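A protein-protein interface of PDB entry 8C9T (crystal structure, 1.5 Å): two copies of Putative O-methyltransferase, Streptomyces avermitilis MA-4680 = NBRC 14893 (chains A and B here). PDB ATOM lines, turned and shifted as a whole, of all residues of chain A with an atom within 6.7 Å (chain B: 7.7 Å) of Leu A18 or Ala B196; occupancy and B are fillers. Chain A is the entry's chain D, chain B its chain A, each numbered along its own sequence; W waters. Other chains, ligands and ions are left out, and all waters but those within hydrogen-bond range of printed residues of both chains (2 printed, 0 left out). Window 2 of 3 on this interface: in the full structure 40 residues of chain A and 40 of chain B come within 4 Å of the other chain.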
ATOM      1  N   ASP A  13      16.477 -14.379   3.348  1.00  0.00           N
ATOM      2  CA  ASP A  13      17.445 -15.013   2.446  1.00  0.00           C
ATOM      3  C   ASP A  13      16.831 -16.334   1.913  1.00  0.00           C
ATOM      4  O   ASP A  13      16.969 -16.655   0.744  1.00  0.00           O
ATOM      5  CB  ASP A  13      18.792 -15.181   3.170  1.00  0.00           C
ATOM      6  CG  ASP A  13      19.823 -15.902   2.341  1.00  0.00           C
ATOM      7  OD1 ASP A  13      20.281 -15.326   1.357  1.00  0.00           O
ATOM      8  OD2 ASP A  13      20.074 -17.110   2.648  1.00  0.00           O
ATOM      9  N   TYR A  14      16.173 -17.082   2.777  1.00  0.00           N
ATOM     10  CA  TYR A  14      15.498 -18.341   2.372  1.00  0.00           C
ATOM     11  C   TYR A  14      14.413 -18.047   1.330  1.00  0.00           C
ATOM     12  O   TYR A  14      14.362 -18.685   0.278  1.00  0.00           O
ATOM     13  CB  TYR A  14      14.925 -19.025   3.588  1.00  0.00           C
ATOM     14  CG  TYR A  14      13.962 -20.127   3.254  1.00  0.00           C
ATOM     15  CD1 TYR A  14      14.443 -21.338   2.799  1.00  0.00           C
ATOM     16  CD2 TYR A  14      12.599 -19.956   3.388  1.00  0.00           C
ATOM     17  CE1 TYR A  14      13.570 -22.359   2.458  1.00  0.00           C
ATOM     18  CE2 TYR A  14      11.719 -20.954   3.014  1.00  0.00           C
ATOM     19  CZ  TYR A  14      12.215 -22.177   2.608  1.00  0.00           C
ATOM     20  OH  TYR A  14      11.344 -23.186   2.245  1.00  0.00           O
ATOM     21  N   PHE A  15      13.569 -17.051   1.574  1.00  0.00           N
ATOM     22  CA  PHE A  15      12.496 -16.735   0.599  1.00  0.00           C
ATOM     23  C   PHE A  15      13.103 -16.242  -0.731  1.00  0.00           C
ATOM     24  O   PHE A  15      12.584 -16.500  -1.809  1.00  0.00           O
ATOM     25  CB  PHE A  15      11.523 -15.721   1.190  1.00  0.00           C
ATOM     26  CG  PHE A  15      10.574 -16.192   2.280  1.00  0.00           C
ATOM     27  CD1 PHE A  15      10.248 -17.527   2.438  1.00  0.00           C
ATOM     28  CD2 PHE A  15      10.045 -15.288   3.163  1.00  0.00           C
ATOM     29  CE1 PHE A  15       9.347 -17.938   3.410  1.00  0.00           C
ATOM     30  CE2 PHE A  15       9.143 -15.687   4.135  1.00  0.00           C
ATOM     31  CZ  PHE A  15       8.801 -17.018   4.271  1.00  0.00           C
ATOM     32  N   THR A  16      14.108 -15.378  -0.609  1.00  0.00           N
ATOM     33  CA  THR A  16      14.759 -14.770  -1.779  1.00  0.00           C
ATOM     34  C   THR A  16      15.360 -15.882  -2.639  1.00  0.00           C
ATOM     35  O   THR A  16      15.038 -15.965  -3.827  1.00  0.00           O
ATOM     36  CB  THR A  16      15.790 -13.720  -1.321  1.00  0.00           C
ATOM     37  OG1 THR A  16      15.047 -12.616  -0.790  1.00  0.00           O
ATOM     38  CG2 THR A  16      16.677 -13.284  -2.464  1.00  0.00           C
ATOM     39  N   THR A  17      16.213 -16.720  -2.072  1.00  0.00           N
ATOM     40  CA  THR A  17      16.927 -17.734  -2.878  1.00  0.00           C
ATOM     41  C   THR A  17      15.936 -18.738  -3.456  1.00  0.00           C
ATOM     42  O   THR A  17      16.144 -19.191  -4.583  1.00  0.00           O
ATOM     43  CB  THR A  17      18.028 -18.418  -2.077  1.00  0.00           C
ATOM     44  OG1 THR A  17      17.529 -19.075  -0.921  1.00  0.00           O
ATOM     45  CG2 THR A  17      19.080 -17.464  -1.585  1.00  0.00           C
ATOM     46  N   LEU A  18      14.821 -19.023  -2.772  1.00  0.00           N
ATOM     47  CA  LEU A  18      13.842 -19.993  -3.300  1.00  0.00           C
ATOM     48  C   LEU A  18      12.956 -19.383  -4.384  1.00  0.00           C
ATOM     49  O   LEU A  18      12.797 -19.981  -5.457  1.00  0.00           O
ATOM     50  CB  LEU A  18      13.033 -20.495  -2.110  1.00  0.00           C
ATOM     51  CG  LEU A  18      11.998 -21.552  -2.466  1.00  0.00           C
ATOM     52  CD1 LEU A  18      12.590 -22.789  -3.152  1.00  0.00           C
ATOM     53  CD2 LEU A  18      11.252 -21.938  -1.206  1.00  0.00           C
ATOM     54  N   LEU A  19      12.356 -18.235  -4.076  1.00  0.00           N
ATOM     55  CA  LEU A  19      11.218 -17.688  -4.829  1.00  0.00           C
ATOM     56  C   LEU A  19      11.566 -16.470  -5.691  1.00  0.00           C
ATOM     57  O   LEU A  19      10.864 -16.267  -6.682  1.00  0.00           O
ATOM     58  CB  LEU A  19      10.089 -17.294  -3.872  1.00  0.00           C
ATOM     59  CG  LEU A  19       9.425 -18.485  -3.190  1.00  0.00           C
ATOM     60  CD1 LEU A  19       8.911 -18.116  -1.798  1.00  0.00           C
ATOM     61  CD2 LEU A  19       8.345 -19.081  -4.065  1.00  0.00           C
ATOM     62  N   ALA A  20      12.482 -15.631  -5.221  1.00  0.00           N
ATOM     63  CA  ALA A  20      12.655 -14.280  -5.798  1.00  0.00           C
ATOM     64  C   ALA A  20      14.123 -13.932  -5.823  1.00  0.00           C
ATOM     65  O   ALA A  20      14.559 -13.037  -5.144  1.00  0.00           O
ATOM     66  CB  ALA A  20      11.897 -13.324  -4.952  1.00  0.00           C
ATOM     67  N   PRO A  21      14.938 -14.698  -6.558  1.00  0.00           N
ATOM     68  CA  PRO A  21      16.386 -14.538  -6.427  1.00  0.00           C
ATOM     69  C   PRO A  21      16.988 -13.189  -6.888  1.00  0.00           C
ATOM     70  O   PRO A  21      16.408 -12.626  -7.764  1.00  0.00           O
ATOM     71  CB  PRO A  21      16.945 -15.693  -7.277  1.00  0.00           C
ATOM     72  CG  PRO A  21      15.788 -16.230  -8.078  1.00  0.00           C
ATOM     73  CD  PRO A  21      14.496 -15.782  -7.432  1.00  0.00           C
ATOM     74  N   VAL B 175      10.773 -22.240   9.120  1.00  0.00           N
ATOM     75  CA  VAL B 175      10.650 -22.648   7.713  1.00  0.00           C
ATOM     76  C   VAL B 175      12.012 -22.778   7.030  1.00  0.00           C
ATOM     77  O   VAL B 175      12.102 -23.498   6.062  1.00  0.00           O
ATOM     78  CB  VAL B 175       9.753 -21.650   6.936  1.00  0.00           C
ATOM     79  CG1 VAL B 175      10.414 -20.310   6.686  1.00  0.00           C
ATOM     80  CG2 VAL B 175       9.201 -22.239   5.668  1.00  0.00           C
ATOM     81  N   THR B 188       5.096 -26.916   4.740  1.00  0.00           N
ATOM     82  CA  THR B 188       5.215 -25.513   4.290  1.00  0.00           C
ATOM     83  C   THR B 188       6.351 -25.427   3.253  1.00  0.00           C
ATOM     84  O   THR B 188       6.178 -24.847   2.172  1.00  0.00           O
ATOM     85  CB  THR B 188       5.523 -24.579   5.455  1.00  0.00           C
ATOM     86  OG1 THR B 188       4.461 -24.643   6.415  1.00  0.00           O
ATOM     87  CG2 THR B 188       5.639 -23.157   4.949  1.00  0.00           C
ATOM     88  N   ARG B 189       7.504 -26.000   3.569  1.00  0.00           N
ATOM     89  CA  ARG B 189       8.686 -25.923   2.682  1.00  0.00           C
ATOM     90  C   ARG B 189       8.339 -26.574   1.343  1.00  0.00           C
ATOM     91  O   ARG B 189       8.625 -25.997   0.287  1.00  0.00           O
ATOM     92  CB  ARG B 189       9.897 -26.592   3.336  1.00  0.00           C
ATOM     93  CG  ARG B 189      10.498 -25.781   4.471  1.00  0.00           C
ATOM     94  CD  ARG B 189      11.588 -26.572   5.204  1.00  0.00           C
ATOM     95  NE  ARG B 189      12.643 -27.053   4.314  1.00  0.00           N
ATOM     96  CZ  ARG B 189      13.713 -26.358   3.939  1.00  0.00           C
ATOM     97  NH1 ARG B 189      13.934 -25.155   4.422  1.00  0.00           N
ATOM     98  NH2 ARG B 189      14.596 -26.928   3.122  1.00  0.00           N
ATOM     99  N   SER B 190       7.710 -27.748   1.357  1.00  0.00           N
ATOM    100  CA  SER B 190       7.342 -28.456   0.115  1.00  0.00           C
ATOM    101  C   SER B 190       6.410 -27.568  -0.697  1.00  0.00           C
ATOM    102  O   SER B 190       6.520 -27.515  -1.918  1.00  0.00           O
ATOM    103  CB  SER B 190       6.726 -29.786   0.442  1.00  0.00           C
ATOM    104  OG  SER B 190       7.698 -30.608   1.033  1.00  0.00           O
ATOM    105  N   ALA B 191       5.481 -26.869  -0.061  1.00  0.00           N
ATOM    106  CA  ALA B 191       4.499 -26.058  -0.792  1.00  0.00           C
ATOM    107  C   ALA B 191       5.210 -24.846  -1.394  1.00  0.00           C
ATOM    108  O   ALA B 191       4.963 -24.528  -2.572  1.00  0.00           O
ATOM    109  CB  ALA B 191       3.406 -25.634   0.145  1.00  0.00           C
ATOM    110  N   LEU B 192       6.143 -24.220  -0.667  1.00  0.00           N
ATOM    111  CA  LEU B 192       6.893 -23.067  -1.228  1.00  0.00           C
ATOM    112  C   LEU B 192       7.813 -23.527  -2.358  1.00  0.00           C
ATOM    113  O   LEU B 192       7.977 -22.812  -3.365  1.00  0.00           O
ATOM    114  CB  LEU B 192       7.699 -22.403  -0.130  1.00  0.00           C
ATOM    115  CG  LEU B 192       6.870 -21.776   0.994  1.00  0.00           C
ATOM    116  CD1 LEU B 192       7.806 -21.199   2.033  1.00  0.00           C
ATOM    117  CD2 LEU B 192       5.932 -20.707   0.462  1.00  0.00           C
ATOM    118  N   GLU B 193       8.378 -24.707  -2.234  1.00  0.00           N
ATOM    119  CA  GLU B 193       9.257 -25.260  -3.288  1.00  0.00           C
ATOM    120  C   GLU B 193       8.426 -25.510  -4.538  1.00  0.00           C
ATOM    121  O   GLU B 193       8.909 -25.245  -5.623  1.00  0.00           O
ATOM    122  CB  GLU B 193       9.923 -26.547  -2.838  1.00  0.00           C
ATOM    123  CG  GLU B 193      10.943 -26.299  -1.762  1.00  0.00           C
ATOM    124  CD  GLU B 193      11.449 -27.561  -1.075  1.00  0.00           C
ATOM    125  OE1 GLU B 193      11.177 -28.685  -1.600  1.00  0.00           O
ATOM    126  OE2 GLU B 193      12.008 -27.449   0.015  1.00  0.00           O
ATOM    127  N   LEU B 194       7.208 -26.000  -4.403  1.00  0.00           N
ATOM    128  CA  LEU B 194       6.348 -26.262  -5.565  1.00  0.00           C
ATOM    129  C   LEU B 194       6.016 -24.924  -6.250  1.00  0.00           C
ATOM    130  O   LEU B 194       6.078 -24.823  -7.502  1.00  0.00           O
ATOM    131  CB  LEU B 194       5.094 -26.995  -5.104  1.00  0.00           C
ATOM    132  CG  LEU B 194       4.058 -27.240  -6.186  1.00  0.00           C
ATOM    133  CD1 LEU B 194       4.667 -28.068  -7.291  1.00  0.00           C
ATOM    134  CD2 LEU B 194       2.859 -27.943  -5.563  1.00  0.00           C
ATOM    135  N   ILE B 195       5.703 -23.876  -5.502  1.00  0.00           N
ATOM    136  CA  ILE B 195       5.451 -22.530  -6.096  1.00  0.00           C
ATOM    137  C   ILE B 195       6.694 -22.071  -6.852  1.00  0.00           C
ATOM    138  O   ILE B 195       6.610 -21.649  -8.041  1.00  0.00           O
ATOM    139  CB  ILE B 195       5.020 -21.553  -5.002  1.00  0.00           C
ATOM    140  CG1 ILE B 195       3.635 -21.963  -4.490  1.00  0.00           C
ATOM    141  CG2 ILE B 195       5.045 -20.131  -5.508  1.00  0.00           C
ATOM    142  CD1 ILE B 195       3.181 -21.130  -3.298  1.00  0.00           C
ATOM    143  N   ALA B 196       7.847 -22.185  -6.206  1.00  0.00           N
ATOM    144  CA  ALA B 196       9.102 -21.690  -6.802  1.00  0.00           C
ATOM    145  C   ALA B 196       9.417 -22.470  -8.073  1.00  0.00           C
ATOM    146  O   ALA B 196       9.747 -21.835  -9.117  1.00  0.00           O
ATOM    147  CB  ALA B 196      10.203 -21.839  -5.816  1.00  0.00           C
ATOM    148  N   GLU B 197       9.215 -23.776  -8.105  1.00  0.00           N
ATOM    149  CA  GLU B 197       9.759 -24.662  -9.153  1.00  0.00           C
ATOM    150  C   GLU B 197       8.750 -24.861 -10.278  1.00  0.00           C
ATOM    151  O   GLU B 197       9.159 -25.157 -11.418  1.00  0.00           O
ATOM    152  CB  GLU B 197      10.176 -25.972  -8.494  1.00  0.00           C
ATOM    153  CG  GLU B 197      11.349 -25.731  -7.576  1.00  0.00           C
ATOM    154  CD  GLU B 197      11.675 -26.859  -6.608  1.00  0.00           C
ATOM    155  OE1 GLU B 197      11.019 -27.905  -6.716  1.00  0.00           O
ATOM    156  OE2 GLU B 197      12.645 -26.708  -5.815  1.00  0.00           O
ATOM    157  N   HIS B 198       7.452 -24.743 -10.008  1.00  0.00           N
ATOM    158  CA  HIS B 198       6.438 -25.061 -11.021  1.00  0.00           C
ATOM    159  C   HIS B 198       6.508 -24.020 -12.117  1.00  0.00           C
ATOM    160  O   HIS B 198       6.481 -22.830 -11.863  1.00  0.00           O
ATOM    161  CB  HIS B 198       5.030 -25.158 -10.418  1.00  0.00           C
ATOM    162  CG  HIS B 198       4.107 -25.879 -11.336  1.00  0.00           C
ATOM    163  ND1 HIS B 198       3.719 -25.322 -12.534  1.00  0.00           N
ATOM    164  CD2 HIS B 198       3.583 -27.126 -11.278  1.00  0.00           C
ATOM    165  CE1 HIS B 198       2.952 -26.187 -13.144  1.00  0.00           C
ATOM    166  NE2 HIS B 198       2.850 -27.295 -12.407  1.00  0.00           N
ATOM    167  N   PRO B 199       6.622 -24.415 -13.400  1.00  0.00           N
ATOM    168  CA  PRO B 199       6.782 -23.409 -14.440  1.00  0.00           C
ATOM    169  C   PRO B 199       5.536 -22.554 -14.709  1.00  0.00           C
ATOM    170  O   PRO B 199       5.711 -21.493 -15.324  1.00  0.00           O
ATOM    171  CB  PRO B 199       7.098 -24.260 -15.685  1.00  0.00           C
ATOM    172  CG  PRO B 199       6.495 -25.578 -15.389  1.00  0.00           C
ATOM    173  CD  PRO B 199       6.707 -25.794 -13.902  1.00  0.00           C
ATOM    174  N   LYS B 200       4.392 -22.947 -14.163  1.00  0.00           N
ATOM    175  CA  LYS B 200       3.146 -22.150 -14.336  1.00  0.00           C
ATOM    176  C   LYS B 200       2.941 -21.221 -13.139  1.00  0.00           C
ATOM    177  O   LYS B 200       1.914 -20.567 -13.131  1.00  0.00           O
ATOM    178  CB  LYS B 200       1.920 -23.052 -14.461  1.00  0.00           C
ATOM    179  CG  LYS B 200       1.804 -23.844 -15.761  1.00  0.00           C
ATOM    180  CD  LYS B 200       0.524 -24.725 -15.857  1.00  0.00           C
ATOM    181  CE  LYS B 200      -0.795 -24.033 -15.529  1.00  0.00           C
ATOM    182  NZ  LYS B 200      -1.203 -23.014 -16.548  1.00  0.00           N
ATOM    183  N   LEU B 201       3.859 -21.138 -12.188  1.00  0.00           N
ATOM    184  CA  LEU B 201       3.670 -20.248 -11.025  1.00  0.00           C
ATOM    185  C   LEU B 201       4.820 -19.271 -10.865  1.00  0.00           C
ATOM    186  O   LEU B 201       5.981 -19.700 -10.922  1.00  0.00           O
ATOM    187  CB  LEU B 201       3.556 -21.084  -9.770  1.00  0.00           C
ATOM    188  CG  LEU B 201       2.296 -21.932  -9.653  1.00  0.00           C
ATOM    189  CD1 LEU B 201       2.332 -22.796  -8.421  1.00  0.00           C
ATOM    190  CD2 LEU B 201       1.064 -21.070  -9.682  1.00  0.00           C
ATOM    191  N   SER B 202       4.514 -18.004 -10.634  1.00  0.00           N
ATOM    192  CA  SER B 202       5.494 -16.952 -10.283  1.00  0.00           C
ATOM    193  C   SER B 202       5.117 -16.491  -8.889  1.00  0.00           C
ATOM    194  O   SER B 202       4.034 -15.944  -8.722  1.00  0.00           O
ATOM    195  CB  SER B 202       5.475 -15.806 -11.286  1.00  0.00           C
ATOM    196  OG  SER B 202       6.395 -14.826 -10.858  1.00  0.00           O
ATOM    197  N   GLY B 203       6.003 -16.602  -7.910  1.00  0.00           N
ATOM    198  CA  GLY B 203       5.610 -16.307  -6.540  1.00  0.00           C
ATOM    199  C   GLY B 203       6.664 -15.590  -5.745  1.00  0.00           C
ATOM    200  O   GLY B 203       7.786 -15.356  -6.217  1.00  0.00           O
ATOM    201  N   THR B 204       6.276 -15.249  -4.542  1.00  0.00           N
ATOM    202  CA  THR B 204       7.168 -14.670  -3.529  1.00  0.00           C
ATOM    203  C   THR B 204       6.566 -14.976  -2.180  1.00  0.00           C
ATOM    204  O   THR B 204       5.455 -15.497  -2.111  1.00  0.00           O
ATOM    205  CB  THR B 204       7.335 -13.149  -3.706  1.00  0.00           C
ATOM    206  OG1 THR B 204       8.491 -12.815  -2.914  1.00  0.00           O
ATOM    207  CG2 THR B 204       6.134 -12.363  -3.267  1.00  0.00           C
ATOM    208  N   ALA B 205       7.313 -14.711  -1.144  1.00  0.00           N
ATOM    209  CA  ALA B 205       6.815 -14.804   0.235  1.00  0.00           C
ATOM    210  C   ALA B 205       7.442 -13.689   1.039  1.00  0.00           C
ATOM    211  O   ALA B 205       8.583 -13.327   0.696  1.00  0.00           O
ATOM    212  CB  ALA B 205       7.149 -16.167   0.798  1.00  0.00           C
ATOM    213  N   ALA B 220       1.295 -16.275  -5.340  1.00  0.00           N
ATOM    214  CA  ALA B 220       1.736 -16.805  -6.641  1.00  0.00           C
ATOM    215  C   ALA B 220       0.702 -16.514  -7.715  1.00  0.00           C
ATOM    216  O   ALA B 220      -0.500 -16.615  -7.461  1.00  0.00           O
ATOM    217  CB  ALA B 220       2.029 -18.271  -6.589  1.00  0.00           C
HETATM  218  O   HOH W   1       8.663 -17.727  -7.840  1.00  0.00           O
HETATM  219  O   HOH W   2      12.641 -25.082   0.989  1.00  0.00           O
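The backbone carbonyl oxygen (O) of Gly B203 lies close to the backbone carbonyl oxygen (O) of Leu A19 (3.2 Å).
O of Tyr A14 lies within hydrogen-bond range of OG1 of Thr A17 (3.4 Å). The backbone carbonyl oxygen (O) of Val B175 sits at hydrogen-bond distance from the guanidinium group (NH1) of Arg B189.
Among the printed residues, pairs that only touch across the chains: Leu A18 with Ala B196 (3.2 Å), Tyr A14 with Arg B189 (3.4 Å), Phe A15 with Ala B205 (3.5 Å), Leu A19 with Ala B205 (3.7 Å), Tyr A14 with Val B175 (3.7 Å), Leu A18 with Leu B192 (3.7 Å), Leu A19 with Ile B195 (3.8 Å), Leu A19 with Ala B196 (3.8 Å), Leu A19 with Leu B192 (3.8 Å), Phe A15 with Leu B192 (3.9 Å) and Leu A19 with Thr B204 (3.9 Å).
Of chain B, only Leu B192 (3.7 Å) and Ala B196 (3.2 Å) come within 4 Å of Leu A18. Ala B196 touches two residues of chain A. Of the printed residues of chain B, Phe A15 touches Leu B192 (3.9 Å) and Ala B205 (3.5 Å). Of the printed residues of chain A, Leu B192 touches Phe A15 (3.9 Å), Leu A18 (3.7 Å) and Leu A19 (3.8 Å). Lys B200 touches none of the printed residues of chain A. His B198 touches none of the printed residues of chain A. The nearest printed residue of chain A that does not touch Ala B196 is Thr A17 (6.6 Å).
Hydrophobic or aromatic side chains of chain B within 4 Å of the printed part of chain A: Val B175, Leu B192, Ile B195, Ala B196 and Ala B205. Printed residues of chain A that touch a printed residue of chain B: Tyr A14, Phe A15, Leu A18 and Leu A19. Hydrophobic or aromatic side chains of chain A that line the printed part of chain B: Tyr A14, Phe A15, Leu A18 and Leu A19.
No position is printed for both chains.
Water W2 lies within hydrogen-bond range of the side-chain hydroxyl of Tyr A14 (2.6 Å), the side-chain carboxylate of Glu B193 (2.6 Å) and the guanidinium group of Arg B189 (3.4 Å). Water W1 lies within hydrogen-bond range of the backbone carbonyl oxygen of Leu A19 (2.9 Å) and the backbone NH of Gly B203 (2.9 Å).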
